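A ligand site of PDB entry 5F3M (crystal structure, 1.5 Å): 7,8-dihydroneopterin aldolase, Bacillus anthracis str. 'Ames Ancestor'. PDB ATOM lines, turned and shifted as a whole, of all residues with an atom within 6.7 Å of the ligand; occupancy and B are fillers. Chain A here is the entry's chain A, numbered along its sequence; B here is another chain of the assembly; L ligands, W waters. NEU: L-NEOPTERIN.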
ATOM      1  N   HIS A  18      14.425  -1.107  -2.813  1.00  0.00           N
ATOM      2  CA  HIS A  18      14.432  -2.556  -2.919  1.00  0.00           C
ATOM      3  C   HIS A  18      14.646  -3.200  -1.550  1.00  0.00           C
ATOM      4  O   HIS A  18      15.278  -2.622  -0.657  1.00  0.00           O
ATOM      5  CB  HIS A  18      15.547  -2.997  -3.861  1.00  0.00           C
ATOM      6  CG  HIS A  18      15.579  -2.203  -5.125  1.00  0.00           C
ATOM      7  ND1 HIS A  18      14.785  -2.500  -6.213  1.00  0.00           N
ATOM      8  CD2 HIS A  18      16.302  -1.105  -5.473  1.00  0.00           C
ATOM      9  CE1 HIS A  18      15.024  -1.626  -7.180  1.00  0.00           C
ATOM     10  NE2 HIS A  18      15.929  -0.764  -6.749  1.00  0.00           N
ATOM     11  N   GLY A  19      14.112  -4.398  -1.387  1.00  0.00           N
ATOM     12  CA  GLY A  19      14.356  -5.151  -0.170  1.00  0.00           C
ATOM     13  C   GLY A  19      13.260  -6.157   0.138  1.00  0.00           C
ATOM     14  O   GLY A  19      12.095  -6.005  -0.240  1.00  0.00           O
ATOM     15  N   VAL A  20      13.641  -7.198   0.879  1.00  0.00           N
ATOM     16  CA  VAL A  20      12.707  -8.240   1.284  1.00  0.00           C
ATOM     17  C   VAL A  20      11.745  -7.728   2.364  1.00  0.00           C
ATOM     18  O   VAL A  20      10.569  -8.101   2.377  1.00  0.00           O
ATOM     19  CB  VAL A  20      13.479  -9.482   1.759  1.00  0.00           C
ATOM     20  CG1 VAL A  20      12.547 -10.506   2.394  1.00  0.00           C
ATOM     21  CG2 VAL A  20      14.254 -10.109   0.601  1.00  0.00           C
ATOM     22  N   PHE A  21      12.247  -6.883   3.288  1.00  0.00           N
ATOM     23  CA  PHE A  21      11.381  -6.445   4.373  1.00  0.00           C
ATOM     24  C   PHE A  21      10.539  -5.256   3.930  1.00  0.00           C
ATOM     25  O   PHE A  21      11.047  -4.322   3.297  1.00  0.00           O
ATOM     26  CB  PHE A  21      12.222  -6.020   5.579  1.00  0.00           C
ATOM     27  CG  PHE A  21      13.031  -7.119   6.183  1.00  0.00           C
ATOM     28  CD1 PHE A  21      12.407  -8.275   6.636  1.00  0.00           C
ATOM     29  CD2 PHE A  21      14.398  -7.007   6.321  1.00  0.00           C
ATOM     30  CE1 PHE A  21      13.146  -9.301   7.203  1.00  0.00           C
ATOM     31  CE2 PHE A  21      15.147  -8.020   6.888  1.00  0.00           C
ATOM     32  CZ  PHE A  21      14.516  -9.170   7.331  1.00  0.00           C
ATOM     33  N   GLU A  24      12.051  -1.868   4.562  1.00  0.00           N
ATOM     34  CA  GLU A  24      13.019  -1.376   3.588  1.00  0.00           C
ATOM     35  C   GLU A  24      12.334  -0.698   2.417  1.00  0.00           C
ATOM     36  O   GLU A  24      12.840   0.292   1.876  1.00  0.00           O
ATOM     37  CB  GLU A  24      13.873  -2.531   3.055  1.00  0.00           C
ATOM     38  CG  GLU A  24      14.814  -3.148   4.063  1.00  0.00           C
ATOM     39  CD  GLU A  24      15.590  -4.292   3.457  1.00  0.00           C
ATOM     40  OE1 GLU A  24      15.036  -5.403   3.364  1.00  0.00           O
ATOM     41  OE2 GLU A  24      16.740  -4.062   3.026  1.00  0.00           O
ATOM     42  N   GLN A  29      17.190   3.070   0.915  1.00  0.00           N
ATOM     43  CA  GLN A  29      18.602   3.021   1.311  1.00  0.00           C
ATOM     44  C   GLN A  29      19.457   3.220   0.067  1.00  0.00           C
ATOM     45  O   GLN A  29      18.965   3.220  -1.060  1.00  0.00           O
ATOM     46  CB  GLN A  29      18.946   1.680   1.984  1.00  0.00           C
ATOM     47  CG  GLN A  29      18.687   0.468   1.107  1.00  0.00           C
ATOM     48  CD  GLN A  29      18.668  -0.825   1.886  1.00  0.00           C
ATOM     49  OE1 GLN A  29      19.693  -1.249   2.435  1.00  0.00           O
ATOM     50  NE2 GLN A  29      17.495  -1.455   1.962  1.00  0.00           N
ATOM     51  N   LYS A  73      12.251  -7.094  -4.563  1.00  0.00           N
ATOM     52  CA  LYS A  73      12.649  -7.621  -3.269  1.00  0.00           C
ATOM     53  C   LYS A  73      14.159  -7.848  -3.198  1.00  0.00           C
ATOM     54  O   LYS A  73      14.794  -7.518  -2.186  1.00  0.00           O
ATOM     55  CB  LYS A  73      11.898  -8.914  -2.946  1.00  0.00           C
ATOM     56  CG  LYS A  73      10.412  -8.725  -2.709  1.00  0.00           C
ATOM     57  CD  LYS A  73       9.727 -10.042  -2.364  1.00  0.00           C
ATOM     58  CE  LYS A  73       8.226  -9.873  -2.221  1.00  0.00           C
ATOM     59  NZ  LYS A  73       7.870  -8.934  -1.128  1.00  0.00           N
ATOM     60  N   LEU A  74      14.748  -8.409  -4.260  1.00  0.00           N
ATOM     61  CA  LEU A  74      16.114  -8.914  -4.228  1.00  0.00           C
ATOM     62  C   LEU A  74      17.075  -8.052  -5.029  1.00  0.00           C
ATOM     63  O   LEU A  74      16.730  -7.573  -6.119  1.00  0.00           O
ATOM     64  CB  LEU A  74      16.179 -10.323  -4.825  1.00  0.00           C
ATOM     65  CG  LEU A  74      15.322 -11.386  -4.164  1.00  0.00           C
ATOM     66  CD1 LEU A  74      15.613 -12.743  -4.810  1.00  0.00           C
ATOM     67  CD2 LEU A  74      15.563 -11.396  -2.657  1.00  0.00           C
ATOM     68  N   VAL A  75      18.296  -7.903  -4.514  1.00  0.00           N
ATOM     69  CA  VAL A  75      19.346  -7.295  -5.333  1.00  0.00           C
ATOM     70  C   VAL A  75      19.641  -8.148  -6.565  1.00  0.00           C
ATOM     71  O   VAL A  75      20.053  -7.629  -7.607  1.00  0.00           O
ATOM     72  CB  VAL A  75      20.604  -6.976  -4.505  1.00  0.00           C
ATOM     73  CG1 VAL A  75      20.324  -5.826  -3.542  1.00  0.00           C
ATOM     74  CG2 VAL A  75      21.095  -8.199  -3.761  1.00  0.00           C
ATOM     75  N   GLU A  76      19.436  -9.477  -6.465  1.00  0.00           N
ATOM     76  CA  GLU A  76      19.555 -10.355  -7.628  1.00  0.00           C
ATOM     77  C   GLU A  76      18.706  -9.848  -8.799  1.00  0.00           C
ATOM     78  O   GLU A  76      19.153  -9.887  -9.959  1.00  0.00           O
ATOM     79  CB  GLU A  76      19.133 -11.778  -7.266  1.00  0.00           C
ATOM     80  CG  GLU A  76      20.162 -12.561  -6.464  1.00  0.00           C
ATOM     81  CD  GLU A  76      20.060 -12.360  -4.953  1.00  0.00           C
ATOM     82  OE1 GLU A  76      20.566 -13.243  -4.230  1.00  0.00           O
ATOM     83  OE2 GLU A  76      19.491 -11.345  -4.474  1.00  0.00           O
ATOM     84  N   LYS A 102      24.714  -3.431  -1.709  1.00  0.00           N
ATOM     85  CA  LYS A 102      23.857  -2.859  -0.687  1.00  0.00           C
ATOM     86  C   LYS A 102      24.780  -2.548   0.478  1.00  0.00           C
ATOM     87  O   LYS A 102      25.168  -3.459   1.229  1.00  0.00           O
ATOM     88  CB  LYS A 102      22.822  -3.906  -0.283  1.00  0.00           C
ATOM     89  CG  LYS A 102      21.542  -3.394   0.294  1.00  0.00           C
ATOM     90  CD  LYS A 102      20.524  -4.523   0.285  1.00  0.00           C
ATOM     91  CE  LYS A 102      19.264  -4.139   0.986  1.00  0.00           C
ATOM     92  NZ  LYS A 102      18.320  -5.274   1.078  1.00  0.00           N
ATOM     93  N   PRO A 105      22.654  -2.497   4.568  1.00  0.00           N
ATOM     94  CA  PRO A 105      21.508  -3.403   4.787  1.00  0.00           C
ATOM     95  C   PRO A 105      21.150  -3.478   6.262  1.00  0.00           C
ATOM     96  O   PRO A 105      21.963  -3.126   7.141  1.00  0.00           O
ATOM     97  CB  PRO A 105      22.046  -4.753   4.304  1.00  0.00           C
ATOM     98  CG  PRO A 105      23.495  -4.682   4.709  1.00  0.00           C
ATOM     99  CD  PRO A 105      23.906  -3.272   4.398  1.00  0.00           C
ATOM    100  N   PRO A 106      19.961  -3.971   6.589  1.00  0.00           N
ATOM    101  CA  PRO A 106      19.523  -4.071   7.990  1.00  0.00           C
ATOM    102  C   PRO A 106      20.038  -5.329   8.700  1.00  0.00           C
ATOM    103  O   PRO A 106      19.276  -6.105   9.267  1.00  0.00           O
ATOM    104  CB  PRO A 106      17.998  -4.066   7.865  1.00  0.00           C
ATOM    105  CG  PRO A 106      17.751  -4.769   6.533  1.00  0.00           C
ATOM    106  CD  PRO A 106      18.868  -4.286   5.636  1.00  0.00           C
ATOM    107  N   ILE A 107      21.355  -5.516   8.667  1.00  0.00           N
ATOM    108  CA  ILE A 107      22.028  -6.652   9.276  1.00  0.00           C
ATOM    109  C   ILE A 107      22.766  -6.149  10.517  1.00  0.00           C
ATOM    110  O   ILE A 107      23.706  -5.356  10.384  1.00  0.00           O
ATOM    111  CB  ILE A 107      23.009  -7.335   8.313  1.00  0.00           C
ATOM    112  CG1 ILE A 107      22.291  -7.847   7.069  1.00  0.00           C
ATOM    113  CG2 ILE A 107      23.758  -8.472   9.014  1.00  0.00           C
ATOM    114  CD1 ILE A 107      23.226  -8.277   5.943  1.00  0.00           C
ATOM    115  N   VAL A 114      27.237  -5.808   1.499  1.00  0.00           N
ATOM    116  CA  VAL A 114      26.903  -7.073   0.857  1.00  0.00           C
ATOM    117  C   VAL A 114      26.654  -6.786  -0.622  1.00  0.00           C
ATOM    118  O   VAL A 114      26.330  -5.666  -1.025  1.00  0.00           O
ATOM    119  CB  VAL A 114      25.684  -7.767   1.509  1.00  0.00           C
ATOM    120  CG1 VAL A 114      25.923  -7.972   3.010  1.00  0.00           C
ATOM    121  CG2 VAL A 114      24.394  -6.968   1.270  1.00  0.00           C
ATOM    122  N   VAL A 116      25.775  -8.746  -4.815  1.00  0.00           N
ATOM    123  CA  VAL A 116      25.663  -9.841  -5.788  1.00  0.00           C
ATOM    124  C   VAL A 116      26.365  -9.425  -7.070  1.00  0.00           C
ATOM    125  O   VAL A 116      26.441  -8.239  -7.409  1.00  0.00           O
ATOM    126  CB  VAL A 116      24.200 -10.251  -6.070  1.00  0.00           C
ATOM    127  CG1 VAL A 116      23.526 -10.849  -4.841  1.00  0.00           C
ATOM    128  CG2 VAL A 116      23.399  -9.083  -6.633  1.00  0.00           C
ATOM    129  N   ILE B   7      27.661 -14.201  -4.476  1.00  0.00           N
ATOM    130  CA  ILE B   7      27.297 -13.324  -3.368  1.00  0.00           C
ATOM    131  C   ILE B   7      28.571 -12.982  -2.621  1.00  0.00           C
ATOM    132  O   ILE B   7      29.403 -13.858  -2.352  1.00  0.00           O
ATOM    133  CB  ILE B   7      26.264 -13.973  -2.424  1.00  0.00           C
ATOM    134  CG1 ILE B   7      24.922 -14.152  -3.128  1.00  0.00           C
ATOM    135  CG2 ILE B   7      26.128 -13.155  -1.131  1.00  0.00           C
ATOM    136  CD1 ILE B   7      23.959 -15.104  -2.408  1.00  0.00           C
ATOM    137  N   LEU B  41      22.449 -17.582  -9.607  1.00  0.00           N
ATOM    138  CA  LEU B  41      21.511 -16.554  -9.163  1.00  0.00           C
ATOM    139  C   LEU B  41      20.408 -16.254 -10.178  1.00  0.00           C
ATOM    140  O   LEU B  41      19.532 -15.429  -9.872  1.00  0.00           O
ATOM    141  CB  LEU B  41      22.251 -15.263  -8.791  1.00  0.00           C
ATOM    142  CG  LEU B  41      23.180 -15.369  -7.582  1.00  0.00           C
ATOM    143  CD1 LEU B  41      23.927 -14.049  -7.351  1.00  0.00           C
ATOM    144  CD2 LEU B  41      22.413 -15.807  -6.343  1.00  0.00           C
ATOM    145  N   LEU B  50      13.488 -15.019  -2.729  1.00  0.00           N
ATOM    146  CA  LEU B  50      14.687 -15.328  -1.965  1.00  0.00           C
ATOM    147  C   LEU B  50      14.910 -16.825  -1.767  1.00  0.00           C
ATOM    148  O   LEU B  50      16.045 -17.239  -1.541  1.00  0.00           O
ATOM    149  CB  LEU B  50      14.624 -14.614  -0.607  1.00  0.00           C
ATOM    150  CG  LEU B  50      15.822 -14.754   0.333  1.00  0.00           C
ATOM    151  CD1 LEU B  50      17.101 -14.230  -0.318  1.00  0.00           C
ATOM    152  CD2 LEU B  50      15.554 -14.036   1.649  1.00  0.00           C
ATOM    153  N   SER B  53      17.729 -18.250  -3.721  1.00  0.00           N
ATOM    154  CA  SER B  53      19.087 -17.783  -3.458  1.00  0.00           C
ATOM    155  C   SER B  53      19.458 -18.196  -2.033  1.00  0.00           C
ATOM    156  O   SER B  53      18.856 -19.089  -1.428  1.00  0.00           O
ATOM    157  CB  SER B  53      19.213 -16.278  -3.737  1.00  0.00           C
ATOM    158  OG  SER B  53      20.565 -15.876  -3.638  1.00  0.00           O
ATOM    159  N   VAL B  54      20.473 -17.528  -1.481  1.00  0.00           N
ATOM    160  CA  VAL B  54      20.928 -17.757  -0.115  1.00  0.00           C
ATOM    161  C   VAL B  54      20.907 -16.413   0.608  1.00  0.00           C
ATOM    162  O   VAL B  54      21.464 -15.434   0.120  1.00  0.00           O
ATOM    163  CB  VAL B  54      22.336 -18.387  -0.078  1.00  0.00           C
ATOM    164  CG1 VAL B  54      22.876 -18.414   1.344  1.00  0.00           C
ATOM    165  CG2 VAL B  54      22.300 -19.809  -0.682  1.00  0.00           C
ATOM    166  N   ASN B  55      20.254 -16.391   1.772  1.00  0.00           N
ATOM    167  CA  ASN B  55      20.084 -15.169   2.547  1.00  0.00           C
ATOM    168  C   ASN B  55      21.437 -14.694   3.069  1.00  0.00           C
ATOM    169  O   ASN B  55      22.072 -15.358   3.895  1.00  0.00           O
ATOM    170  CB  ASN B  55      19.154 -15.502   3.712  1.00  0.00           C
ATOM    171  CG  ASN B  55      18.711 -14.279   4.478  1.00  0.00           C
ATOM    172  OD1 ASN B  55      19.478 -13.337   4.684  1.00  0.00           O
ATOM    173  ND2 ASN B  55      17.450 -14.282   4.927  1.00  0.00           N
ATOM    174  N   TYR B  56      21.899 -13.523   2.615  1.00  0.00           N
ATOM    175  CA  TYR B  56      23.237 -13.105   3.027  1.00  0.00           C
ATOM    176  C   TYR B  56      23.325 -12.740   4.501  1.00  0.00           C
ATOM    177  O   TYR B  56      24.424 -12.759   5.065  1.00  0.00           O
ATOM    178  CB  TYR B  56      23.865 -12.043   2.111  1.00  0.00           C
ATOM    179  CG  TYR B  56      22.979 -10.891   1.732  1.00  0.00           C
ATOM    180  CD1 TYR B  56      22.359 -10.104   2.703  1.00  0.00           C
ATOM    181  CD2 TYR B  56      22.777 -10.573   0.401  1.00  0.00           C
ATOM    182  CE1 TYR B  56      21.538  -9.036   2.326  1.00  0.00           C
ATOM    183  CE2 TYR B  56      21.976  -9.529   0.025  1.00  0.00           C
ATOM    184  CZ  TYR B  56      21.365  -8.764   0.993  1.00  0.00           C
ATOM    185  OH  TYR B  56      20.567  -7.716   0.595  1.00  0.00           O
ATOM    186  N   GLY B  57      22.200 -12.439   5.158  1.00  0.00           N
ATOM    187  CA  GLY B  57      22.234 -12.233   6.590  1.00  0.00           C
ATOM    188  C   GLY B  57      22.610 -13.502   7.337  1.00  0.00           C
ATOM    189  O   GLY B  57      23.295 -13.454   8.365  1.00  0.00           O
ATOM    190  N   GLU B  58      22.155 -14.657   6.839  1.00  0.00           N
ATOM    191  CA  GLU B  58      22.559 -15.930   7.424  1.00  0.00           C
ATOM    192  C   GLU B  58      24.046 -16.172   7.210  1.00  0.00           C
ATOM    193  O   GLU B  58      24.720 -16.725   8.091  1.00  0.00           O
ATOM    194  CB  GLU B  58      21.734 -17.071   6.840  1.00  0.00           C
ATOM    195  CG  GLU B  58      20.258 -17.031   7.197  1.00  0.00           C
ATOM    196  CD  GLU B  58      19.476 -18.193   6.594  1.00  0.00           C
ATOM    197  OE1 GLU B  58      18.234 -18.187   6.712  1.00  0.00           O
ATOM    198  OE2 GLU B  58      20.094 -19.101   5.991  1.00  0.00           O
HETATM  199  N2  NEU L   1      19.511 -11.157  -1.649  1.00  0.00           N
HETATM  200  C1  NEU L   1      18.820 -10.144  -1.111  1.00  0.00           C
HETATM  201  C10 NEU L   1      18.550 -10.181   0.337  1.00  0.00           C
HETATM  202  N9  NEU L   1      17.867  -9.211   0.986  1.00  0.00           N
HETATM  203  C8  NEU L   1      17.683  -9.336   2.323  1.00  0.00           C
HETATM  204  C7  NEU L   1      18.172 -10.438   3.005  1.00  0.00           C
HETATM  205  N6  NEU L   1      18.857 -11.408   2.408  1.00  0.00           N
HETATM  206  C5  NEU L   1      19.085 -11.334   1.092  1.00  0.00           C
HETATM  207  N4  NEU L   1      19.771 -12.284   0.434  1.00  0.00           N
HETATM  208  C3  NEU L   1      19.974 -12.191  -0.910  1.00  0.00           C
HETATM  209  N13 NEU L   1      20.679 -13.171  -1.510  1.00  0.00           N
HETATM  210  C16 NEU L   1      16.979  -8.264   3.068  1.00  0.00           C
HETATM  211  O21 NEU L   1      16.302  -7.370   2.163  1.00  0.00           O
HETATM  212  C26 NEU L   1      18.026  -7.380   3.802  1.00  0.00           C
HETATM  213  O22 NEU L   1      19.034  -6.852   2.902  1.00  0.00           O
HETATM  214  C28 NEU L   1      18.829  -7.992   4.960  1.00  0.00           C
HETATM  215  O24 NEU L   1      17.982  -8.698   5.864  1.00  0.00           O
HETATM  216  O11 NEU L   1      18.405  -9.187  -1.808  1.00  0.00           O
HETATM  217  O   HOH W   1      16.599 -11.709   6.306  1.00  0.00           O
HETATM  218  O   HOH W   2      18.533  -8.681   8.732  1.00  0.00           O
HETATM  219  O   HOH W   3      17.328  -6.787  -1.231  1.00  0.00           O
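The side-chain amino group (NZ) of Lys 102 sits at hydrogen-bond distance from an oxygen (O22) of the ligand (2.5 Å).
The side-chain carboxylate (OE1) of Glu 24 is in hydrogen-bond range of an oxygen (O21) of the ligand (2.6 Å).
N13 of the ligand lies within hydrogen-bond range of OE1 of Glu 76 (2.7 Å).
The backbone carbonyl oxygen (O) of Val 54 of chain B sits at hydrogen-bond distance from a nitrogen (N13) of the ligand (2.9 Å).
A nitrogen (N4) of the ligand is in hydrogen-bond range of the backbone NH (N) of Tyr 56 of chain B, 3.3 Å away.
The side-chain hydroxyl (OH) of Tyr 56 of chain B lies within hydrogen-bond range of an oxygen (O22) of the ligand.
The backbone NH (N) of Val 20 sits at hydrogen-bond distance from an oxygen (O21) of the ligand (3.0 Å).
An oxygen (O11) of the ligand is in hydrogen-bond range of the backbone NH of Val 75 (3.0 Å).
OD1 of Asn 55 of chain B sits close to N6 of the ligand, 3.0 Å away.
The side-chain hydroxyl (OG) of Ser 53 of chain B sits at hydrogen-bond distance from a nitrogen (N13) of the ligand.
The side-chain carboxylate of Glu 24 is in salt-bridge range of the side-chain amino group of Lys 102 (2.8 Å).
The side-chain hydroxyl of Tyr 56 of chain B sits close to the side-chain amino group of Lys 102.
The backbone NH (N) of Lys 102 lies within hydrogen-bond range of the backbone carbonyl oxygen (O) of Val 114 (2.8 Å).
The side-chain carboxylate (OE1) of Glu 24 sits at hydrogen-bond distance from the backbone NH (N) of Val 20 (3.4 Å).
The side-chain carboxylate of Glu 24 sits at hydrogen-bond distance from the backbone NH of Phe 21 (3.2 Å).
The side-chain carboxylate (OE2) of Glu 24 lies within hydrogen-bond range of the side-chain amide nitrogen (NE2) of Gln 29, at 2.9 Å.
The side-chain carboxylate (OE1) of Glu 76 is in hydrogen-bond range of the side-chain hydroxyl (OG) of Ser 53 of chain B (2.7 Å).
O of Lys 73 lies close to N of Gly 19.
CA of Gly 19 touches O21 of the ligand, 3.8 Å away.
CE2 of Phe 21 touches O24 of the ligand (3.1 Å).
Lys 73 touches the ligand (O to O11, 3.996 Å).
CA of Leu 74 touches O11 of the ligand, at 3.3 Å.
Pro 105 touches the ligand.
CD of Pro 106 touches C26 of the ligand, 3.7 Å away.
Ile 7 of chain B touches the ligand (CD1 to N13, 3.9 Å).
CD1 of Leu 50 of chain B touches N4 of the ligand, at 3.4 Å.
17 residues have an atom within 4 Å of the ligand: Gly 19, Val 20, Phe 21, Glu 24, Lys 73, Leu 74, Val 75, Glu 76, Lys 102, Pro 105, Pro 106, Ile 7 of chain B, Leu 50 of chain B, Ser 53 of chain B, Val 54 of chain B, Asn 55 of chain B and Tyr 56 of chain B.
Water W3 lies within hydrogen-bond range of O11 of the ligand, O of Lys 73 and NZ of Lys 102.
Water W2 lies within hydrogen-bond range of O of Pro 106 (2.7 Å) and O24 of the ligand (2.9 Å).
Water W1 bridges ND2 of Asn 55 of chain B (3.0 Å) and O24 of the ligand (3.3 Å).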
